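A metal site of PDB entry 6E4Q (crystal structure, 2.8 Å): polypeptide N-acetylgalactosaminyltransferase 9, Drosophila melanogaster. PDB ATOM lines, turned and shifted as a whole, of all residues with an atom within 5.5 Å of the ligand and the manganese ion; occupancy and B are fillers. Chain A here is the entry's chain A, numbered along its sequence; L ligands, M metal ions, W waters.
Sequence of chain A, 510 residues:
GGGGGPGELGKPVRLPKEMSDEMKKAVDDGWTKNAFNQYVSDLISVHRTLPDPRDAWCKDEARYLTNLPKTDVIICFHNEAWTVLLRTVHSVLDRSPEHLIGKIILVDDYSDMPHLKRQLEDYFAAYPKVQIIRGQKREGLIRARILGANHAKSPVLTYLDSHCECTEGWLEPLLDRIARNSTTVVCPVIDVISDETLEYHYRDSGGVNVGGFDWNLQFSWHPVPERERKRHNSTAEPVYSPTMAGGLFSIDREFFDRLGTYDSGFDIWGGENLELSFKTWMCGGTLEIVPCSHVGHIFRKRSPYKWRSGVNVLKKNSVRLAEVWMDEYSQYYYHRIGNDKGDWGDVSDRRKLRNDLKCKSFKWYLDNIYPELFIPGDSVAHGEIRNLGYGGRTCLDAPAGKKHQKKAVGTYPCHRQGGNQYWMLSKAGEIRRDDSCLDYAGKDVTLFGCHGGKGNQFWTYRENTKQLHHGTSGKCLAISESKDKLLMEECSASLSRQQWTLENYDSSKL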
ATOM      1  N   ILE A  75     -18.225  21.985 -35.499  1.00  0.00           N
ATOM      2  CA  ILE A  75     -17.727  22.587 -34.255  1.00  0.00           C
ATOM      3  C   ILE A  75     -18.554  22.012 -33.108  1.00  0.00           C
ATOM      4  O   ILE A  75     -19.682  22.454 -32.861  1.00  0.00           O
ATOM      5  CB  ILE A  75     -17.831  24.117 -34.292  1.00  0.00           C
ATOM      6  CG1 ILE A  75     -17.296  24.685 -35.601  1.00  0.00           C
ATOM      7  CG2 ILE A  75     -17.095  24.733 -33.096  1.00  0.00           C
ATOM      8  CD1 ILE A  75     -17.527  26.185 -35.767  1.00  0.00           C
ATOM      9  N   CYS A  76     -18.010  21.059 -32.355  1.00  0.00           N
ATOM     10  CA  CYS A  76     -18.738  20.654 -31.149  1.00  0.00           C
ATOM     11  C   CYS A  76     -18.502  21.655 -30.013  1.00  0.00           C
ATOM     12  O   CYS A  76     -17.495  22.382 -29.999  1.00  0.00           O
ATOM     13  CB  CYS A  76     -18.333  19.267 -30.695  1.00  0.00           C
ATOM     14  SG  CYS A  76     -18.498  17.974 -31.947  1.00  0.00           S
ATOM     15  N   PHE A  77     -19.441  21.706 -29.075  1.00  0.00           N
ATOM     16  CA  PHE A  77     -19.306  22.636 -27.952  1.00  0.00           C
ATOM     17  C   PHE A  77     -20.131  22.153 -26.765  1.00  0.00           C
ATOM     18  O   PHE A  77     -20.983  21.277 -26.903  1.00  0.00           O
ATOM     19  CB  PHE A  77     -19.693  24.068 -28.355  1.00  0.00           C
ATOM     20  CG  PHE A  77     -21.132  24.228 -28.731  1.00  0.00           C
ATOM     21  CD1 PHE A  77     -21.547  23.973 -30.019  1.00  0.00           C
ATOM     22  CD2 PHE A  77     -22.063  24.670 -27.793  1.00  0.00           C
ATOM     23  CE1 PHE A  77     -22.881  24.136 -30.368  1.00  0.00           C
ATOM     24  CE2 PHE A  77     -23.392  24.829 -28.120  1.00  0.00           C
ATOM     25  CZ  PHE A  77     -23.805  24.567 -29.415  1.00  0.00           C
ATOM     26  N   HIS A  78     -19.835  22.690 -25.584  1.00  0.00           N
ATOM     27  CA  HIS A  78     -20.638  22.470 -24.377  1.00  0.00           C
ATOM     28  C   HIS A  78     -20.425  23.655 -23.445  1.00  0.00           C
ATOM     29  O   HIS A  78     -19.326  23.828 -22.915  1.00  0.00           O
ATOM     30  CB  HIS A  78     -20.258  21.176 -23.653  1.00  0.00           C
ATOM     31  CG  HIS A  78     -20.964  21.016 -22.332  1.00  0.00           C
ATOM     32  ND1 HIS A  78     -22.131  20.311 -22.179  1.00  0.00           N
ATOM     33  CD2 HIS A  78     -20.662  21.511 -21.104  1.00  0.00           C
ATOM     34  CE1 HIS A  78     -22.522  20.358 -20.927  1.00  0.00           C
ATOM     35  NE2 HIS A  78     -21.653  21.085 -20.246  1.00  0.00           N
ATOM     36  N   GLU A  80     -20.042  26.650 -24.214  1.00  0.00           N
ATOM     37  CA  GLU A  80     -19.077  27.592 -24.748  1.00  0.00           C
ATOM     38  C   GLU A  80     -19.581  29.034 -24.636  1.00  0.00           C
ATOM     39  O   GLU A  80     -20.787  29.296 -24.656  1.00  0.00           O
ATOM     40  CB  GLU A  80     -18.749  27.271 -26.208  1.00  0.00           C
ATOM     41  CG  GLU A  80     -17.660  28.164 -26.775  1.00  0.00           C
ATOM     42  CD  GLU A  80     -16.394  28.126 -25.935  1.00  0.00           C
ATOM     43  OE1 GLU A  80     -15.452  27.367 -26.276  1.00  0.00           O
ATOM     44  OE2 GLU A  80     -16.344  28.850 -24.905  1.00  0.00           O
ATOM     45  N   ASP A 109     -24.213  18.910 -27.714  1.00  0.00           N
ATOM     46  CA  ASP A 109     -23.793  18.078 -26.551  1.00  0.00           C
ATOM     47  C   ASP A 109     -24.349  18.582 -25.214  1.00  0.00           C
ATOM     48  O   ASP A 109     -23.620  18.754 -24.220  1.00  0.00           O
ATOM     49  CB  ASP A 109     -22.276  17.934 -26.462  1.00  0.00           C
ATOM     50  CG  ASP A 109     -21.870  16.823 -25.495  1.00  0.00           C
ATOM     51  OD1 ASP A 109     -22.680  15.901 -25.339  1.00  0.00           O
ATOM     52  OD2 ASP A 109     -20.777  16.878 -24.888  1.00  0.00           O
ATOM     53  N   ARG A 138     -25.582  14.596 -22.417  1.00  0.00           N
ATOM     54  CA  ARG A 138     -24.153  14.827 -22.504  1.00  0.00           C
ATOM     55  C   ARG A 138     -23.471  13.521 -22.879  1.00  0.00           C
ATOM     56  O   ARG A 138     -23.643  12.495 -22.220  1.00  0.00           O
ATOM     57  CB  ARG A 138     -23.604  15.373 -21.194  1.00  0.00           C
ATOM     58  CG  ARG A 138     -22.102  15.694 -21.146  1.00  0.00           C
ATOM     59  CD  ARG A 138     -21.736  17.076 -21.674  1.00  0.00           C
ATOM     60  NE  ARG A 138     -20.416  17.448 -21.168  1.00  0.00           N
ATOM     61  CZ  ARG A 138     -20.245  17.992 -19.956  1.00  0.00           C
ATOM     62  NH1 ARG A 138     -19.034  18.302 -19.492  1.00  0.00           N
ATOM     63  NH2 ARG A 138     -21.315  18.203 -19.182  1.00  0.00           N
ATOM     64  N   GLU A 139     -22.721  13.550 -23.968  1.00  0.00           N
ATOM     65  CA  GLU A 139     -22.104  12.353 -24.472  1.00  0.00           C
ATOM     66  C   GLU A 139     -20.629  12.541 -24.736  1.00  0.00           C
ATOM     67  O   GLU A 139     -19.944  11.548 -25.031  1.00  0.00           O
ATOM     68  CB  GLU A 139     -22.781  11.899 -25.782  1.00  0.00           C
ATOM     69  CG  GLU A 139     -24.203  11.379 -25.601  1.00  0.00           C
ATOM     70  CD  GLU A 139     -24.309   9.852 -25.748  1.00  0.00           C
ATOM     71  OE1 GLU A 139     -24.951   9.399 -26.712  1.00  0.00           O
ATOM     72  OE2 GLU A 139     -23.724   9.121 -24.908  1.00  0.00           O
ATOM     73  N   GLY A 140     -20.123  13.759 -24.622  1.00  0.00           N
ATOM     74  CA  GLY A 140     -18.716  14.003 -24.823  1.00  0.00           C
ATOM     75  C   GLY A 140     -18.352  14.300 -26.267  1.00  0.00           C
ATOM     76  O   GLY A 140     -19.108  14.085 -27.212  1.00  0.00           O
ATOM     77  N   LEU A 141     -17.124  14.765 -26.413  1.00  0.00           N
ATOM     78  CA  LEU A 141     -16.592  15.171 -27.705  1.00  0.00           C
ATOM     79  C   LEU A 141     -16.651  14.054 -28.749  1.00  0.00           C
ATOM     80  O   LEU A 141     -17.125  14.270 -29.877  1.00  0.00           O
ATOM     81  CB  LEU A 141     -15.157  15.644 -27.468  1.00  0.00           C
ATOM     82  CG  LEU A 141     -14.191  15.812 -28.611  1.00  0.00           C
ATOM     83  CD1 LEU A 141     -14.502  17.210 -29.173  1.00  0.00           C
ATOM     84  CD2 LEU A 141     -12.752  15.659 -28.122  1.00  0.00           C
ATOM     85  N   ALA A 144     -20.033  13.275 -30.148  1.00  0.00           N
ATOM     86  CA  ALA A 144     -20.592  14.452 -30.796  1.00  0.00           C
ATOM     87  C   ALA A 144     -20.021  14.654 -32.189  1.00  0.00           C
ATOM     88  O   ALA A 144     -20.751  14.944 -33.141  1.00  0.00           O
ATOM     89  CB  ALA A 144     -20.364  15.697 -29.935  1.00  0.00           C
ATOM     90  N   ARG A 145     -18.697  14.535 -32.329  1.00  0.00           N
ATOM     91  CA  ARG A 145     -18.129  14.627 -33.668  1.00  0.00           C
ATOM     92  C   ARG A 145     -18.729  13.570 -34.598  1.00  0.00           C
ATOM     93  O   ARG A 145     -18.903  13.823 -35.803  1.00  0.00           O
ATOM     94  CB  ARG A 145     -16.607  14.481 -33.635  1.00  0.00           C
ATOM     95  CG  ARG A 145     -15.782  15.587 -32.964  1.00  0.00           C
ATOM     96  CD  ARG A 145     -14.309  15.214 -33.167  1.00  0.00           C
ATOM     97  NE  ARG A 145     -13.358  15.662 -32.141  1.00  0.00           N
ATOM     98  CZ  ARG A 145     -12.897  16.891 -31.982  1.00  0.00           C
ATOM     99  NH1 ARG A 145     -13.298  17.896 -32.744  1.00  0.00           N
ATOM    100  NH2 ARG A 145     -12.017  17.119 -30.998  1.00  0.00           N
ATOM    101  N   LEU A 160     -13.326  21.813 -35.842  1.00  0.00           N
ATOM    102  CA  LEU A 160     -12.720  22.917 -35.110  1.00  0.00           C
ATOM    103  C   LEU A 160     -13.300  22.928 -33.703  1.00  0.00           C
ATOM    104  O   LEU A 160     -14.490  22.679 -33.526  1.00  0.00           O
ATOM    105  CB  LEU A 160     -12.996  24.261 -35.798  1.00  0.00           C
ATOM    106  CG  LEU A 160     -12.494  24.521 -37.221  1.00  0.00           C
ATOM    107  CD1 LEU A 160     -12.967  25.897 -37.632  1.00  0.00           C
ATOM    108  CD2 LEU A 160     -10.998  24.448 -37.337  1.00  0.00           C
ATOM    109  N   ASP A 161     -12.470  23.250 -32.719  1.00  0.00           N
ATOM    110  CA  ASP A 161     -12.979  23.537 -31.390  1.00  0.00           C
ATOM    111  C   ASP A 161     -13.826  24.817 -31.406  1.00  0.00           C
ATOM    112  O   ASP A 161     -13.743  25.623 -32.327  1.00  0.00           O
ATOM    113  CB  ASP A 161     -11.840  23.691 -30.383  1.00  0.00           C
ATOM    114  CG  ASP A 161     -11.205  22.357 -30.038  1.00  0.00           C
ATOM    115  OD1 ASP A 161     -11.437  21.383 -30.792  1.00  0.00           O
ATOM    116  OD2 ASP A 161     -10.480  22.287 -29.017  1.00  0.00           O
ATOM    117  N   SER A 162     -14.649  24.993 -30.383  1.00  0.00           N
ATOM    118  CA  SER A 162     -15.494  26.182 -30.318  1.00  0.00           C
ATOM    119  C   SER A 162     -14.733  27.430 -29.899  1.00  0.00           C
ATOM    120  O   SER A 162     -15.338  28.503 -29.790  1.00  0.00           O
ATOM    121  CB  SER A 162     -16.668  25.954 -29.352  1.00  0.00           C
ATOM    122  OG  SER A 162     -16.205  25.489 -28.118  1.00  0.00           O
ATOM    123  N   HIS A 163     -13.445  27.320 -29.595  1.00  0.00           N
ATOM    124  CA  HIS A 163     -12.685  28.506 -29.248  1.00  0.00           C
ATOM    125  C   HIS A 163     -11.499  28.653 -30.198  1.00  0.00           C
ATOM    126  O   HIS A 163     -10.344  28.608 -29.777  1.00  0.00           O
ATOM    127  CB  HIS A 163     -12.244  28.440 -27.777  1.00  0.00           C
ATOM    128  CG  HIS A 163     -11.860  27.065 -27.344  1.00  0.00           C
ATOM    129  ND1 HIS A 163     -12.783  26.112 -26.962  1.00  0.00           N
ATOM    130  CD2 HIS A 163     -10.639  26.479 -27.219  1.00  0.00           C
ATOM    131  CE1 HIS A 163     -12.153  24.992 -26.647  1.00  0.00           C
ATOM    132  NE2 HIS A 163     -10.851  25.192 -26.785  1.00  0.00           N
ATOM    133  N   ILE A 268     -15.330   9.419 -22.493  1.00  0.00           N
ATOM    134  CA  ILE A 268     -14.987  10.822 -22.764  1.00  0.00           C
ATOM    135  C   ILE A 268     -13.468  11.085 -22.740  1.00  0.00           C
ATOM    136  O   ILE A 268     -12.942  11.832 -23.576  1.00  0.00           O
ATOM    137  CB  ILE A 268     -15.736  11.745 -21.786  1.00  0.00           C
ATOM    138  CG1 ILE A 268     -17.242  11.513 -21.928  1.00  0.00           C
ATOM    139  CG2 ILE A 268     -15.326  13.212 -21.991  1.00  0.00           C
ATOM    140  CD1 ILE A 268     -18.099  12.601 -21.352  1.00  0.00           C
ATOM    141  N   HIS A 297      -6.193  29.009 -31.529  1.00  0.00           N
ATOM    142  CA  HIS A 297      -6.939  28.241 -30.538  1.00  0.00           C
ATOM    143  C   HIS A 297      -6.679  28.852 -29.163  1.00  0.00           C
ATOM    144  O   HIS A 297      -5.555  29.320 -28.887  1.00  0.00           O
ATOM    145  CB  HIS A 297      -6.550  26.757 -30.579  1.00  0.00           C
ATOM    146  CG  HIS A 297      -7.030  25.944 -29.412  1.00  0.00           C
ATOM    147  ND1 HIS A 297      -6.161  25.389 -28.485  1.00  0.00           N
ATOM    148  CD2 HIS A 297      -8.263  25.547 -29.037  1.00  0.00           C
ATOM    149  CE1 HIS A 297      -6.852  24.710 -27.580  1.00  0.00           C
ATOM    150  NE2 HIS A 297      -8.127  24.793 -27.896  1.00  0.00           N
ATOM    151  N   ILE A 298      -7.704  28.890 -28.323  1.00  0.00           N
ATOM    152  CA  ILE A 298      -7.566  29.386 -26.954  1.00  0.00           C
ATOM    153  C   ILE A 298      -7.095  28.216 -26.079  1.00  0.00           C
ATOM    154  O   ILE A 298      -7.874  27.358 -25.690  1.00  0.00           O
ATOM    155  CB  ILE A 298      -8.872  29.976 -26.424  1.00  0.00           C
ATOM    156  CG1 ILE A 298      -9.327  31.138 -27.299  1.00  0.00           C
ATOM    157  CG2 ILE A 298      -8.704  30.437 -24.974  1.00  0.00           C
ATOM    158  CD1 ILE A 298     -10.385  32.001 -26.646  1.00  0.00           C
ATOM    159  N   ARG A 300      -6.130  26.455 -22.718  1.00  0.00           N
ATOM    160  CA  ARG A 300      -6.558  26.604 -21.331  1.00  0.00           C
ATOM    161  C   ARG A 300      -5.669  25.753 -20.416  1.00  0.00           C
ATOM    162  O   ARG A 300      -5.197  24.686 -20.801  1.00  0.00           O
ATOM    163  CB  ARG A 300      -7.995  26.157 -21.142  1.00  0.00           C
ATOM    164  CG  ARG A 300      -9.047  26.794 -22.006  1.00  0.00           C
ATOM    165  CD  ARG A 300     -10.379  26.534 -21.317  1.00  0.00           C
ATOM    166  NE  ARG A 300     -11.577  26.448 -22.149  1.00  0.00           N
ATOM    167  CZ  ARG A 300     -11.986  25.347 -22.768  1.00  0.00           C
ATOM    168  NH1 ARG A 300     -11.258  24.239 -22.698  1.00  0.00           N
ATOM    169  NH2 ARG A 300     -13.113  25.373 -23.475  1.00  0.00           N
ATOM    170  N   SER A 303      -9.631  22.093 -17.919  1.00  0.00           N
ATOM    171  CA  SER A 303     -10.956  21.976 -18.545  1.00  0.00           C
ATOM    172  C   SER A 303     -12.047  22.002 -17.478  1.00  0.00           C
ATOM    173  O   SER A 303     -11.967  21.247 -16.497  1.00  0.00           O
ATOM    174  CB  SER A 303     -11.071  20.683 -19.352  1.00  0.00           C
ATOM    175  OG  SER A 303     -11.705  19.671 -18.587  1.00  0.00           O
ATOM    176  N   TYR A 305     -15.088  20.788 -17.152  1.00  0.00           N
ATOM    177  CA  TYR A 305     -16.145  19.850 -17.524  1.00  0.00           C
ATOM    178  C   TYR A 305     -16.410  18.861 -16.398  1.00  0.00           C
ATOM    179  O   TYR A 305     -15.523  18.533 -15.611  1.00  0.00           O
ATOM    180  CB  TYR A 305     -15.756  19.099 -18.793  1.00  0.00           C
ATOM    181  CG  TYR A 305     -15.508  20.004 -19.959  1.00  0.00           C
ATOM    182  CD1 TYR A 305     -16.353  21.066 -20.230  1.00  0.00           C
ATOM    183  CD2 TYR A 305     -14.413  19.794 -20.800  1.00  0.00           C
ATOM    184  CE1 TYR A 305     -16.124  21.903 -21.301  1.00  0.00           C
ATOM    185  CE2 TYR A 305     -14.172  20.628 -21.879  1.00  0.00           C
ATOM    186  CZ  TYR A 305     -15.033  21.684 -22.119  1.00  0.00           C
ATOM    187  OH  TYR A 305     -14.800  22.515 -23.183  1.00  0.00           O
HETATM  188  N1  LIG L   1     -16.693  19.733 -25.787  1.00  0.00           N
HETATM  189  C1  LIG L   1     -17.613  18.786 -26.198  1.00  0.00           C
HETATM  190  N2  LIG L   1     -18.196  17.933 -25.275  1.00  0.00           N
HETATM  191  C2  LIG L   1     -17.868  18.022 -23.940  1.00  0.00           C
HETATM  192  C3  LIG L   1     -16.935  18.982 -23.554  1.00  0.00           C
HETATM  193  C4  LIG L   1     -16.170  19.608 -24.537  1.00  0.00           C
HETATM  194  O1  LIG L   1     -17.906  18.710 -27.393  1.00  0.00           O
HETATM  195  O2  LIG L   1     -18.397  17.257 -23.117  1.00  0.00           O
HETATM  196  C5  LIG L   1     -16.110  20.618 -26.835  1.00  0.00           C
HETATM  197  C6  LIG L   1     -15.632  21.996 -26.386  1.00  0.00           C
HETATM  198  O3  LIG L   1     -16.655  22.983 -26.335  1.00  0.00           O
HETATM  199  C7  LIG L   1     -14.552  22.297 -27.424  1.00  0.00           C
HETATM  200  C8  LIG L   1     -14.110  20.960 -28.005  1.00  0.00           C
HETATM  201  O4  LIG L   1     -15.005  19.992 -27.474  1.00  0.00           O
HETATM  202  O5  LIG L   1     -15.085  23.067 -28.478  1.00  0.00           O
HETATM  203  C9  LIG L   1     -12.682  20.584 -27.634  1.00  0.00           C
HETATM  204  O6  LIG L   1     -12.612  20.448 -26.233  1.00  0.00           O
HETATM  205  P1  LIG L   1     -11.469  21.145 -25.328  1.00  0.00           P
HETATM  206  O7  LIG L   1     -11.119  22.470 -25.863  1.00  0.00           O
HETATM  207  O8  LIG L   1     -11.941  21.295 -23.930  1.00  0.00           O
HETATM  208  O9  LIG L   1     -10.194  20.177 -25.472  1.00  0.00           O
HETATM  209  P2  LIG L   1      -8.671  20.736 -25.516  1.00  0.00           P
HETATM  210  O10 LIG L   1      -8.445  21.459 -26.804  1.00  0.00           O
HETATM  211  O11 LIG L   1      -8.477  21.667 -24.370  1.00  0.00           O
HETATM  212  O12 LIG L   1      -7.741  19.569 -25.448  1.00  0.00           O
HETATM  213 MN    MN M   1      -9.676  23.295 -27.206  1.00  0.00          MN
HETATM  214  O   HOH W   1      -9.640  24.661 -25.010  1.00  0.00           O
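Water W1 lies within hydrogen-bond range of the guanidinium group of Arg 300 (2.9 Å), an oxygen (O11) of the ligand (3.3 Å) and the backbone carbonyl oxygen of Ile 298 (3.3 Å).
The manganese ion is bound by O7 of the ligand (2.1 Å), OD2 of Asp 161 (2.2 Å), O10 of the ligand (2.2 Å), NE2 of His 297 (2.3 Å), NE2 of His 163 (2.3 Å) and water W1 (2.6 Å). The manganese ion has six donor atoms within binding distance.
N of Arg 145 is in hydrogen-bond range of SG of Cys 76. The side-chain carboxylate of Asp 109 is in hydrogen-bond range of the backbone NH of Glu 139 (2.7 Å). The guanidinium group of Arg 138 lies within salt-bridge range of the side-chain carboxylate of Asp 109 (3.8 Å). A ring nitrogen (NE2) of His 78 lies close to the guanidinium group of Arg 138 (3.1 Å). The side-chain hydroxyl of Tyr 305 sits at hydrogen-bond distance from the guanidinium group of Arg 300, 3.3 Å away. A ring nitrogen (ND1) of His 163 lies within hydrogen-bond range of the side-chain carboxylate of Glu 80 (3.0 Å). N of Gly 140 sits at hydrogen-bond distance from OD2 of Asp 109 (3.2 Å). The backbone carbonyl oxygen (O) of His 163 is in hydrogen-bond range of the backbone NH (N) of Ile 298, at 3.0 Å.
The nearest printed residue that does not touch the manganese ion is Ile 298 (4.7 Å).
Merely in contact with the ligand: Phe 77, Leu 141 and Gly 140. Hydrophobic or aromatic side chains that line the ligand: Phe 77, His 78, Leu 141, His 163, His 297 and Tyr 305. Of the 22 residues printed, 13 come within 4 Å of the ligand. The nearest printed residue that does not touch the ligand is Glu 80 (4.5 Å).
The backbone NH (N) of Ser 162 is in hydrogen-bond range of an oxygen (O5) of the ligand. O of Cys 76 is in hydrogen-bond range of O5 of the ligand (2.9 Å). NE of Arg 138 sits at hydrogen-bond distance from O2 of the ligand (2.8 Å). O3 of the ligand lies within hydrogen-bond range of N of His 78. An oxygen (O5) of the ligand sits at hydrogen-bond distance from the side-chain hydroxyl (OG) of Ser 162, 2.7 Å away. OH of Tyr 305 lies close to O8 of the ligand. The side-chain carboxylate (OD2) of Asp 109 is in hydrogen-bond range of a nitrogen (N2) of the ligand, at 2.8 Å. NH1 of Arg 300 is in salt-bridge range of O8 of the ligand (3.3 Å).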
